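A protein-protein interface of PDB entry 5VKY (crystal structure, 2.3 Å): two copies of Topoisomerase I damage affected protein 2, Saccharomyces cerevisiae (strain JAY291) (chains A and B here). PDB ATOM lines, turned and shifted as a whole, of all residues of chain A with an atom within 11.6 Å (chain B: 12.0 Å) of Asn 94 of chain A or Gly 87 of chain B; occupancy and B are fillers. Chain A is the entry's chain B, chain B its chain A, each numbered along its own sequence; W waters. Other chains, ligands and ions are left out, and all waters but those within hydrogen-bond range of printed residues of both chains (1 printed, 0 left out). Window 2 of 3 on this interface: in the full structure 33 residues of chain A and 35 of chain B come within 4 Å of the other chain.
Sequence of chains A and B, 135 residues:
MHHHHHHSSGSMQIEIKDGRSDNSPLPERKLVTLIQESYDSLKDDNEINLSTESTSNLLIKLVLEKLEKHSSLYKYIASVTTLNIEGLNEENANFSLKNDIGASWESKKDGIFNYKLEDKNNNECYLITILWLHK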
ATOM      1  N   LEU A  83     -12.043  17.526  -2.976  1.00  0.00           N
ATOM      2  CA  LEU A  83     -13.379  17.361  -2.427  1.00  0.00           C
ATOM      3  C   LEU A  83     -14.160  16.441  -3.354  1.00  0.00           C
ATOM      4  O   LEU A  83     -14.266  16.714  -4.554  1.00  0.00           O
ATOM      5  CB  LEU A  83     -14.068  18.722  -2.291  1.00  0.00           C
ATOM      6  CG  LEU A  83     -15.555  18.659  -1.952  1.00  0.00           C
ATOM      7  CD1 LEU A  83     -15.725  18.074  -0.548  1.00  0.00           C
ATOM      8  CD2 LEU A  83     -16.210  20.040  -2.093  1.00  0.00           C
ATOM      9  N   ASN A  84     -14.689  15.342  -2.818  1.00  0.00           N
ATOM     10  CA  ASN A  84     -15.597  14.520  -3.628  1.00  0.00           C
ATOM     11  C   ASN A  84     -17.013  14.552  -3.057  1.00  0.00           C
ATOM     12  O   ASN A  84     -17.227  14.099  -1.939  1.00  0.00           O
ATOM     13  CB  ASN A  84     -15.101  13.072  -3.723  1.00  0.00           C
ATOM     14  CG  ASN A  84     -15.821  12.268  -4.824  1.00  0.00           C
ATOM     15  OD1 ASN A  84     -16.998  12.505  -5.133  1.00  0.00           O
ATOM     16  ND2 ASN A  84     -15.099  11.324  -5.429  1.00  0.00           N
ATOM     17  N   ALA A  93     -26.003  20.760  -5.466  1.00  0.00           N
ATOM     18  CA  ALA A  93     -25.525  21.042  -4.114  1.00  0.00           C
ATOM     19  C   ALA A  93     -24.927  22.443  -4.029  1.00  0.00           C
ATOM     20  O   ALA A  93     -24.463  22.990  -5.033  1.00  0.00           O
ATOM     21  CB  ALA A  93     -24.501  20.000  -3.688  1.00  0.00           C
ATOM     22  N   ASN A  94     -24.946  23.022  -2.829  1.00  0.00           N
ATOM     23  CA  ASN A  94     -24.370  24.344  -2.580  1.00  0.00           C
ATOM     24  C   ASN A  94     -23.218  24.186  -1.590  1.00  0.00           C
ATOM     25  O   ASN A  94     -23.430  23.970  -0.393  1.00  0.00           O
ATOM     26  CB  ASN A  94     -25.421  25.327  -2.064  1.00  0.00           C
ATOM     27  CG  ASN A  94     -26.761  25.194  -2.780  1.00  0.00           C
ATOM     28  OD1 ASN A  94     -26.927  25.666  -3.907  1.00  0.00           O
ATOM     29  ND2 ASN A  94     -27.727  24.568  -2.116  1.00  0.00           N
ATOM     30  N   PHE A  95     -21.996  24.281  -2.096  1.00  0.00           N
ATOM     31  CA  PHE A  95     -20.800  24.252  -1.272  1.00  0.00           C
ATOM     32  C   PHE A  95     -19.872  25.354  -1.749  1.00  0.00           C
ATOM     33  O   PHE A  95     -19.913  25.754  -2.917  1.00  0.00           O
ATOM     34  CB  PHE A  95     -20.067  22.928  -1.383  1.00  0.00           C
ATOM     35  CG  PHE A  95     -19.641  22.623  -2.776  1.00  0.00           C
ATOM     36  CD1 PHE A  95     -18.346  22.890  -3.194  1.00  0.00           C
ATOM     37  CD2 PHE A  95     -20.558  22.132  -3.696  1.00  0.00           C
ATOM     38  CE1 PHE A  95     -17.962  22.626  -4.500  1.00  0.00           C
ATOM     39  CE2 PHE A  95     -20.187  21.868  -4.992  1.00  0.00           C
ATOM     40  CZ  PHE A  95     -18.886  22.115  -5.399  1.00  0.00           C
ATOM     41  N   SER A  96     -19.036  25.840  -0.842  1.00  0.00           N
ATOM     42  CA  SER A  96     -17.907  26.661  -1.233  1.00  0.00           C
ATOM     43  C   SER A  96     -16.650  26.112  -0.578  1.00  0.00           C
ATOM     44  O   SER A  96     -16.675  25.621   0.554  1.00  0.00           O
ATOM     45  CB  SER A  96     -18.107  28.131  -0.874  1.00  0.00           C
ATOM     46  OG  SER A  96     -18.060  28.344   0.522  1.00  0.00           O
ATOM     47  N   LEU A  97     -15.556  26.189  -1.327  1.00  0.00           N
ATOM     48  CA  LEU A  97     -14.249  25.713  -0.913  1.00  0.00           C
ATOM     49  C   LEU A  97     -13.301  26.896  -0.978  1.00  0.00           C
ATOM     50  O   LEU A  97     -13.124  27.470  -2.052  1.00  0.00           O
ATOM     51  CB  LEU A  97     -13.776  24.591  -1.838  1.00  0.00           C
ATOM     52  CG  LEU A  97     -12.779  23.562  -1.337  1.00  0.00           C
ATOM     53  CD1 LEU A  97     -13.260  22.896  -0.045  1.00  0.00           C
ATOM     54  CD2 LEU A  97     -12.561  22.518  -2.424  1.00  0.00           C
ATOM     55  N   LYS A  98     -12.695  27.258   0.159  1.00  0.00           N
ATOM     56  CA  LYS A  98     -11.747  28.362   0.226  1.00  0.00           C
ATOM     57  C   LYS A  98     -10.450  27.888   0.856  1.00  0.00           C
ATOM     58  O   LYS A  98     -10.418  26.879   1.572  1.00  0.00           O
ATOM     59  CB  LYS A  98     -12.283  29.556   1.041  1.00  0.00           C
ATOM     60  CG  LYS A  98     -13.693  29.986   0.676  1.00  0.00           C
ATOM     61  CD  LYS A  98     -13.663  31.067  -0.384  1.00  0.00           C
ATOM     62  CE  LYS A  98     -15.063  31.567  -0.732  1.00  0.00           C
ATOM     63  NZ  LYS A  98     -15.176  31.795  -2.206  1.00  0.00           N
ATOM     64  N   LYS A 116      -9.105  27.003  -8.698  1.00  0.00           N
ATOM     65  CA  LYS A 116     -10.116  25.987  -8.459  1.00  0.00           C
ATOM     66  C   LYS A 116     -10.404  25.208  -9.737  1.00  0.00           C
ATOM     67  O   LYS A 116     -10.564  25.800 -10.803  1.00  0.00           O
ATOM     68  CB  LYS A 116     -11.409  26.611  -7.926  1.00  0.00           C
ATOM     69  CG  LYS A 116     -12.379  25.551  -7.403  1.00  0.00           C
ATOM     70  CD  LYS A 116     -13.343  26.106  -6.371  1.00  0.00           C
ATOM     71  CE  LYS A 116     -14.375  26.980  -7.046  1.00  0.00           C
ATOM     72  NZ  LYS A 116     -14.827  26.381  -8.329  1.00  0.00           N
ATOM     73  N   GLU A 118     -12.816  21.784 -11.338  1.00  0.00           N
ATOM     74  CA  GLU A 118     -13.969  20.922 -11.107  1.00  0.00           C
ATOM     75  C   GLU A 118     -14.056  19.808 -12.145  1.00  0.00           C
ATOM     76  O   GLU A 118     -13.586  19.934 -13.280  1.00  0.00           O
ATOM     77  CB  GLU A 118     -15.270  21.724 -11.089  1.00  0.00           C
ATOM     78  CG  GLU A 118     -15.596  22.252  -9.709  1.00  0.00           C
ATOM     79  CD  GLU A 118     -16.396  23.540  -9.724  1.00  0.00           C
ATOM     80  OE1 GLU A 118     -16.540  24.155  -8.637  1.00  0.00           O
ATOM     81  OE2 GLU A 118     -16.890  23.929 -10.809  1.00  0.00           O
ATOM     82  N   CYS A 125     -14.033  18.220  -6.854  1.00  0.00           N
ATOM     83  CA  CYS A 125     -13.566  19.596  -6.917  1.00  0.00           C
ATOM     84  C   CYS A 125     -12.132  19.642  -6.398  1.00  0.00           C
ATOM     85  O   CYS A 125     -11.803  18.952  -5.427  1.00  0.00           O
ATOM     86  CB  CYS A 125     -14.480  20.514  -6.082  1.00  0.00           C
ATOM     87  SG  CYS A 125     -14.012  22.255  -6.093  1.00  0.00           S
ATOM     88  N   THR B  82     -11.344  25.838   4.088  1.00  0.00           N
ATOM     89  CA  THR B  82     -12.659  25.970   4.703  1.00  0.00           C
ATOM     90  C   THR B  82     -13.707  25.431   3.739  1.00  0.00           C
ATOM     91  O   THR B  82     -13.860  25.953   2.625  1.00  0.00           O
ATOM     92  CB  THR B  82     -12.951  27.431   5.067  1.00  0.00           C
ATOM     93  OG1 THR B  82     -11.935  27.917   5.948  1.00  0.00           O
ATOM     94  CG2 THR B  82     -14.288  27.568   5.759  1.00  0.00           C
ATOM     95  N   LEU B  83     -14.409  24.378   4.156  1.00  0.00           N
ATOM     96  CA  LEU B  83     -15.560  23.864   3.419  1.00  0.00           C
ATOM     97  C   LEU B  83     -16.824  24.359   4.108  1.00  0.00           C
ATOM     98  O   LEU B  83     -17.012  24.135   5.306  1.00  0.00           O
ATOM     99  CB  LEU B  83     -15.567  22.332   3.349  1.00  0.00           C
ATOM    100  CG  LEU B  83     -16.744  21.661   2.619  1.00  0.00           C
ATOM    101  CD1 LEU B  83     -16.954  22.169   1.164  1.00  0.00           C
ATOM    102  CD2 LEU B  83     -16.607  20.154   2.628  1.00  0.00           C
ATOM    103  N   ASN B  84     -17.667  25.053   3.361  1.00  0.00           N
ATOM    104  CA  ASN B  84     -18.921  25.562   3.893  1.00  0.00           C
ATOM    105  C   ASN B  84     -20.037  24.958   3.061  1.00  0.00           C
ATOM    106  O   ASN B  84     -20.054  25.119   1.837  1.00  0.00           O
ATOM    107  CB  ASN B  84     -18.962  27.089   3.855  1.00  0.00           C
ATOM    108  CG  ASN B  84     -20.292  27.636   4.308  1.00  0.00           C
ATOM    109  OD1 ASN B  84     -21.100  28.092   3.498  1.00  0.00           O
ATOM    110  ND2 ASN B  84     -20.545  27.560   5.612  1.00  0.00           N
ATOM    111  N   ILE B  85     -20.945  24.239   3.704  1.00  0.00           N
ATOM    112  CA  ILE B  85     -22.009  23.559   2.983  1.00  0.00           C
ATOM    113  C   ILE B  85     -23.306  24.326   3.170  1.00  0.00           C
ATOM    114  O   ILE B  85     -23.668  24.698   4.292  1.00  0.00           O
ATOM    115  CB  ILE B  85     -22.138  22.092   3.411  1.00  0.00           C
ATOM    116  CG1 ILE B  85     -20.848  21.364   3.052  1.00  0.00           C
ATOM    117  CG2 ILE B  85     -23.320  21.447   2.714  1.00  0.00           C
ATOM    118  CD1 ILE B  85     -20.634  20.143   3.832  1.00  0.00           C
ATOM    119  N   GLU B  86     -23.977  24.590   2.061  1.00  0.00           N
ATOM    120  CA  GLU B  86     -25.236  25.311   2.016  1.00  0.00           C
ATOM    121  C   GLU B  86     -26.301  24.380   1.447  1.00  0.00           C
ATOM    122  O   GLU B  86     -26.051  23.638   0.480  1.00  0.00           O
ATOM    123  CB  GLU B  86     -25.099  26.556   1.140  1.00  0.00           C
ATOM    124  CG  GLU B  86     -26.357  27.399   0.795  1.00  0.00           C
ATOM    125  CD  GLU B  86     -27.130  28.025   1.968  1.00  0.00           C
ATOM    126  OE1 GLU B  86     -27.055  27.601   3.145  1.00  0.00           O
ATOM    127  OE2 GLU B  86     -27.844  29.000   1.684  1.00  0.00           O
ATOM    128  N   GLY B  87     -27.505  24.434   2.028  1.00  0.00           N
ATOM    129  CA  GLY B  87     -28.637  23.727   1.468  1.00  0.00           C
ATOM    130  C   GLY B  87     -28.881  22.352   2.039  1.00  0.00           C
ATOM    131  O   GLY B  87     -29.779  21.658   1.553  1.00  0.00           O
ATOM    132  N   LEU B  88     -28.106  21.933   3.038  1.00  0.00           N
ATOM    133  CA  LEU B  88     -28.336  20.692   3.769  1.00  0.00           C
ATOM    134  C   LEU B  88     -27.379  20.664   4.944  1.00  0.00           C
ATOM    135  O   LEU B  88     -26.319  21.296   4.914  1.00  0.00           O
ATOM    136  CB  LEU B  88     -28.134  19.448   2.900  1.00  0.00           C
ATOM    137  CG  LEU B  88     -26.709  19.097   2.485  1.00  0.00           C
ATOM    138  CD1 LEU B  88     -26.557  17.588   2.437  1.00  0.00           C
ATOM    139  CD2 LEU B  88     -26.413  19.705   1.135  1.00  0.00           C
ATOM    140  N   ASN B  89     -27.764  19.923   5.981  1.00  0.00           N
ATOM    141  CA  ASN B  89     -26.927  19.849   7.169  1.00  0.00           C
ATOM    142  C   ASN B  89     -25.708  18.975   6.906  1.00  0.00           C
ATOM    143  O   ASN B  89     -25.799  17.906   6.289  1.00  0.00           O
ATOM    144  CB  ASN B  89     -27.724  19.345   8.369  1.00  0.00           C
ATOM    145  CG  ASN B  89     -28.429  20.479   9.101  1.00  0.00           C
ATOM    146  OD1 ASN B  89     -28.612  21.572   8.559  1.00  0.00           O
ATOM    147  ND2 ASN B  89     -28.805  20.229  10.346  1.00  0.00           N
ATOM    148  N   GLU B  90     -24.555  19.465   7.370  1.00  0.00           N
ATOM    149  CA  GLU B  90     -23.269  18.974   6.899  1.00  0.00           C
ATOM    150  C   GLU B  90     -23.010  17.542   7.352  1.00  0.00           C
ATOM    151  O   GLU B  90     -22.291  16.798   6.673  1.00  0.00           O
ATOM    152  CB  GLU B  90     -22.180  19.925   7.385  1.00  0.00           C
ATOM    153  CG  GLU B  90     -20.771  19.448   7.123  1.00  0.00           C
ATOM    154  CD  GLU B  90     -20.007  19.177   8.376  1.00  0.00           C
ATOM    155  OE1 GLU B  90     -19.951  20.087   9.227  1.00  0.00           O
ATOM    156  OE2 GLU B  90     -19.473  18.057   8.513  1.00  0.00           O
ATOM    157  N   GLU B  91     -23.601  17.127   8.477  1.00  0.00           N
ATOM    158  CA  GLU B  91     -23.445  15.762   8.958  1.00  0.00           C
ATOM    159  C   GLU B  91     -24.328  14.765   8.217  1.00  0.00           C
ATOM    160  O   GLU B  91     -24.145  13.558   8.393  1.00  0.00           O
ATOM    161  CB  GLU B  91     -23.738  15.710  10.457  1.00  0.00           C
ATOM    162  CG  GLU B  91     -25.076  16.333  10.880  1.00  0.00           C
ATOM    163  CD  GLU B  91     -25.069  17.866  10.924  1.00  0.00           C
ATOM    164  OE1 GLU B  91     -25.443  18.421  11.978  1.00  0.00           O
ATOM    165  OE2 GLU B  91     -24.720  18.518   9.909  1.00  0.00           O
ATOM    166  N   ASN B  92     -25.287  15.237   7.416  1.00  0.00           N
ATOM    167  CA  ASN B  92     -26.102  14.380   6.563  1.00  0.00           C
ATOM    168  C   ASN B  92     -25.531  14.254   5.157  1.00  0.00           C
ATOM    169  O   ASN B  92     -26.131  13.579   4.312  1.00  0.00           O
ATOM    170  CB  ASN B  92     -27.539  14.913   6.480  1.00  0.00           C
ATOM    171  CG  ASN B  92     -28.266  14.862   7.813  1.00  0.00           C
ATOM    172  OD1 ASN B  92     -27.890  14.103   8.712  1.00  0.00           O
ATOM    173  ND2 ASN B  92     -29.312  15.676   7.950  1.00  0.00           N
ATOM    174  N   ALA B  93     -24.404  14.898   4.883  1.00  0.00           N
ATOM    175  CA  ALA B  93     -23.782  14.856   3.570  1.00  0.00           C
ATOM    176  C   ALA B  93     -22.670  13.823   3.569  1.00  0.00           C
ATOM    177  O   ALA B  93     -21.948  13.670   4.555  1.00  0.00           O
ATOM    178  CB  ALA B  93     -23.225  16.224   3.174  1.00  0.00           C
ATOM    179  N   ASN B  94     -22.542  13.111   2.460  1.00  0.00           N
ATOM    180  CA  ASN B  94     -21.456  12.166   2.263  1.00  0.00           C
ATOM    181  C   ASN B  94     -20.419  12.806   1.343  1.00  0.00           C
ATOM    182  O   ASN B  94     -20.700  13.072   0.166  1.00  0.00           O
ATOM    183  CB  ASN B  94     -21.978  10.848   1.688  1.00  0.00           C
ATOM    184  CG  ASN B  94     -23.240  10.366   2.393  1.00  0.00           C
ATOM    185  OD1 ASN B  94     -23.174   9.720   3.445  1.00  0.00           O
ATOM    186  ND2 ASN B  94     -24.398  10.681   1.816  1.00  0.00           N
ATOM    187  N   PHE B  95     -19.233  13.065   1.887  1.00  0.00           N
ATOM    188  CA  PHE B  95     -18.147  13.654   1.119  1.00  0.00           C
ATOM    189  C   PHE B  95     -16.833  13.265   1.773  1.00  0.00           C
ATOM    190  O   PHE B  95     -16.792  12.881   2.946  1.00  0.00           O
ATOM    191  CB  PHE B  95     -18.284  15.183   1.040  1.00  0.00           C
ATOM    192  CG  PHE B  95     -18.227  15.869   2.388  1.00  0.00           C
ATOM    193  CD1 PHE B  95     -19.384  16.069   3.129  1.00  0.00           C
ATOM    194  CD2 PHE B  95     -17.018  16.306   2.915  1.00  0.00           C
ATOM    195  CE1 PHE B  95     -19.338  16.693   4.369  1.00  0.00           C
ATOM    196  CE2 PHE B  95     -16.964  16.932   4.153  1.00  0.00           C
ATOM    197  CZ  PHE B  95     -18.130  17.123   4.883  1.00  0.00           C
ATOM    198  N   LYS B 120     -20.113  21.224  13.149  1.00  0.00           N
ATOM    199  CA  LYS B 120     -21.402  20.722  12.683  1.00  0.00           C
ATOM    200  C   LYS B 120     -22.477  21.802  12.729  1.00  0.00           C
ATOM    201  O   LYS B 120     -23.333  21.875  11.840  1.00  0.00           O
ATOM    202  CB  LYS B 120     -21.813  19.517  13.525  1.00  0.00           C
ATOM    203  CG  LYS B 120     -21.936  18.224  12.740  1.00  0.00           C
ATOM    204  CD  LYS B 120     -22.688  17.172  13.536  1.00  0.00           C
ATOM    205  CE  LYS B 120     -21.804  15.976  13.845  1.00  0.00           C
ATOM    206  NZ  LYS B 120     -22.608  14.784  14.241  1.00  0.00           N
ATOM    207  N   ASN B 121     -22.432  22.667  13.744  1.00  0.00           N
ATOM    208  CA  ASN B 121     -23.481  23.657  13.954  1.00  0.00           C
ATOM    209  C   ASN B 121     -23.414  24.815  12.972  1.00  0.00           C
ATOM    210  O   ASN B 121     -24.435  25.472  12.745  1.00  0.00           O
ATOM    211  CB  ASN B 121     -23.418  24.197  15.385  1.00  0.00           C
ATOM    212  CG  ASN B 121     -23.940  23.199  16.419  1.00  0.00           C
ATOM    213  OD1 ASN B 121     -24.548  22.184  16.073  1.00  0.00           O
ATOM    214  ND2 ASN B 121     -23.702  23.490  17.694  1.00  0.00           N
ATOM    215  N   ASN B 122     -22.250  25.098  12.392  1.00  0.00           N
ATOM    216  CA  ASN B 122     -22.152  26.129  11.367  1.00  0.00           C
ATOM    217  C   ASN B 122     -22.019  25.543   9.967  1.00  0.00           C
ATOM    218  O   ASN B 122     -21.769  26.289   9.015  1.00  0.00           O
ATOM    219  CB  ASN B 122     -20.991  27.075  11.671  1.00  0.00           C
ATOM    220  CG  ASN B 122     -21.359  28.130  12.706  1.00  0.00           C
ATOM    221  OD1 ASN B 122     -22.511  28.562  12.774  1.00  0.00           O
ATOM    222  ND2 ASN B 122     -20.389  28.537  13.529  1.00  0.00           N
ATOM    223  N   ASN B 123     -22.210  24.228   9.819  1.00  0.00           N
ATOM    224  CA  ASN B 123     -22.115  23.547   8.528  1.00  0.00           C
ATOM    225  C   ASN B 123     -20.768  23.815   7.873  1.00  0.00           C
ATOM    226  O   ASN B 123     -20.680  24.203   6.707  1.00  0.00           O
ATOM    227  CB  ASN B 123     -23.258  23.958   7.604  1.00  0.00           C
ATOM    228  CG  ASN B 123     -24.584  23.437   8.076  1.00  0.00           C
ATOM    229  OD1 ASN B 123     -24.770  22.228   8.195  1.00  0.00           O
ATOM    230  ND2 ASN B 123     -25.510  24.345   8.373  1.00  0.00           N
ATOM    231  N   GLU B 124     -19.707  23.616   8.650  1.00  0.00           N
ATOM    232  CA  GLU B 124     -18.371  23.966   8.205  1.00  0.00           C
ATOM    233  C   GLU B 124     -17.394  22.879   8.603  1.00  0.00           C
ATOM    234  O   GLU B 124     -17.516  22.285   9.674  1.00  0.00           O
ATOM    235  CB  GLU B 124     -17.915  25.304   8.792  1.00  0.00           C
ATOM    236  CG  GLU B 124     -18.107  26.456   7.838  1.00  0.00           C
ATOM    237  CD  GLU B 124     -17.983  27.780   8.533  1.00  0.00           C
ATOM    238  OE1 GLU B 124     -18.193  27.811   9.771  1.00  0.00           O
ATOM    239  OE2 GLU B 124     -17.668  28.778   7.841  1.00  0.00           O
ATOM    240  N   CYS B 125     -16.432  22.634   7.726  1.00  0.00           N
ATOM    241  CA  CYS B 125     -15.340  21.717   7.967  1.00  0.00           C
ATOM    242  C   CYS B 125     -14.046  22.443   7.620  1.00  0.00           C
ATOM    243  O   CYS B 125     -13.992  23.205   6.650  1.00  0.00           O
ATOM    244  CB  CYS B 125     -15.506  20.425   7.132  1.00  0.00           C
ATOM    245  SG  CYS B 125     -14.322  19.115   7.549  1.00  0.00           S
HETATM  246  O   HOH W   1     -15.850  27.883   2.339  1.00  0.00           O
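Of the printed residues of chain B, Leu 83 of chain A touches Leu 83 (3.9 Å). No residue of chain B comes within 4 Å of Ala 93 of chain A. Printed residues of chain B within 4 Å of Asn 94 of chain A: Ile 85 (3.6 Å), Glu 86 (2.6 Å) and Gly 87 (3.8 Å). Of chain B, only Asn 84 (3.3 Å) comes within 4 Å of Phe 95 of chain A. Of chain B, only Thr 82 (3.5 Å), Leu 83 (3.5 Å) and Asn 84 (3.0 Å) come within 4 Å of Ser 96 of chain A. Of the printed residues of chain B, Lys 98 of chain A touches Thr 82. Printed residues of chain A within 4 Å of Thr 82 of chain B: Ser 96 (3.5 Å), Leu 97 (3.6 Å) and Lys 98 (2.9 Å). Of the printed residues of chain A, Ile 85 of chain B touches Asn 94 (3.6 Å). Gly 87 of chain B touches one residue of chain A. Of the printed residues of chain A, Phe 95 of chain B touches Asn 84 (3.2 Å). Glu 124 of chain B touches none of the printed residues of chain A. The nearest residue of chain B that does not touch Asn 94 of chain A is Asn 84 of chain B (4.2 Å). The nearest printed residue of chain B that does not touch Leu 83 of chain A is Phe 95 of chain B (4.1 Å).
O of Cys 125 of chain B is in hydrogen-bond range of N of Leu 83 of chain B (2.8 Å). O of Leu 83 of chain A sits at hydrogen-bond distance from N of Cys 125 of chain A (2.8 Å). N of Ile 85 of chain B lies within hydrogen-bond range of O of Asn 123 of chain B (3.0 Å).
Of the 20 printed residues of chain B, 7 touch a printed residue of chain A. Among the printed residues, 12 pairs touch across the chains.
O of Asn 84 of chain B is in hydrogen-bond range of N of Ser 96 of chain A (3.0 Å). N of Glu 86 of chain B lies within hydrogen-bond range of O of Asn 94 of chain A (2.6 Å). The backbone NH (N) of Thr 82 of chain B sits at hydrogen-bond distance from the backbone carbonyl oxygen (O) of Lys 98 of chain A.
Water W1 bridges O of Thr 82 of chain B (2.8 Å) and OG of Ser 96 of chain A (2.9 Å).
Leu 83 of chain B touches its own counterpart, Leu 83 of chain A. Asn 84 of chain A touches Phe 95 of chain B, and with the chains exchanged Phe 95 of chain A touches Asn 84 of chain B. Positions printed for both chains: 83, 84, 93, 94, 95 and 125. Of the 12 pairs that touch across the chains among the printed residues, 3 have their exchanged pair printed and touching as well.
Leu 83 of chain B touches Leu 83 of chain A. Asn 84 of chain A touches Phe 95 of chain B (O to CA, 3.2 Å). Ile 85 of chain B touches Asn 94 of chain A. CA of Gly 87 of chain B touches ND2 of Asn 94 of chain A (3.8 Å). Asn 84 of chain B touches Phe 95 of chain A (O to CA, 3.3 Å). Thr 82 of chain B touches Ser 96 of chain A (O to O, 3.5 Å). Ser 96 of chain A touches Leu 83 of chain B. Leu 97 of chain A touches Thr 82 of chain B. Leu 83 of chain B touches Leu 97 of chain A (CD1 to CD1, 3.95 Å).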
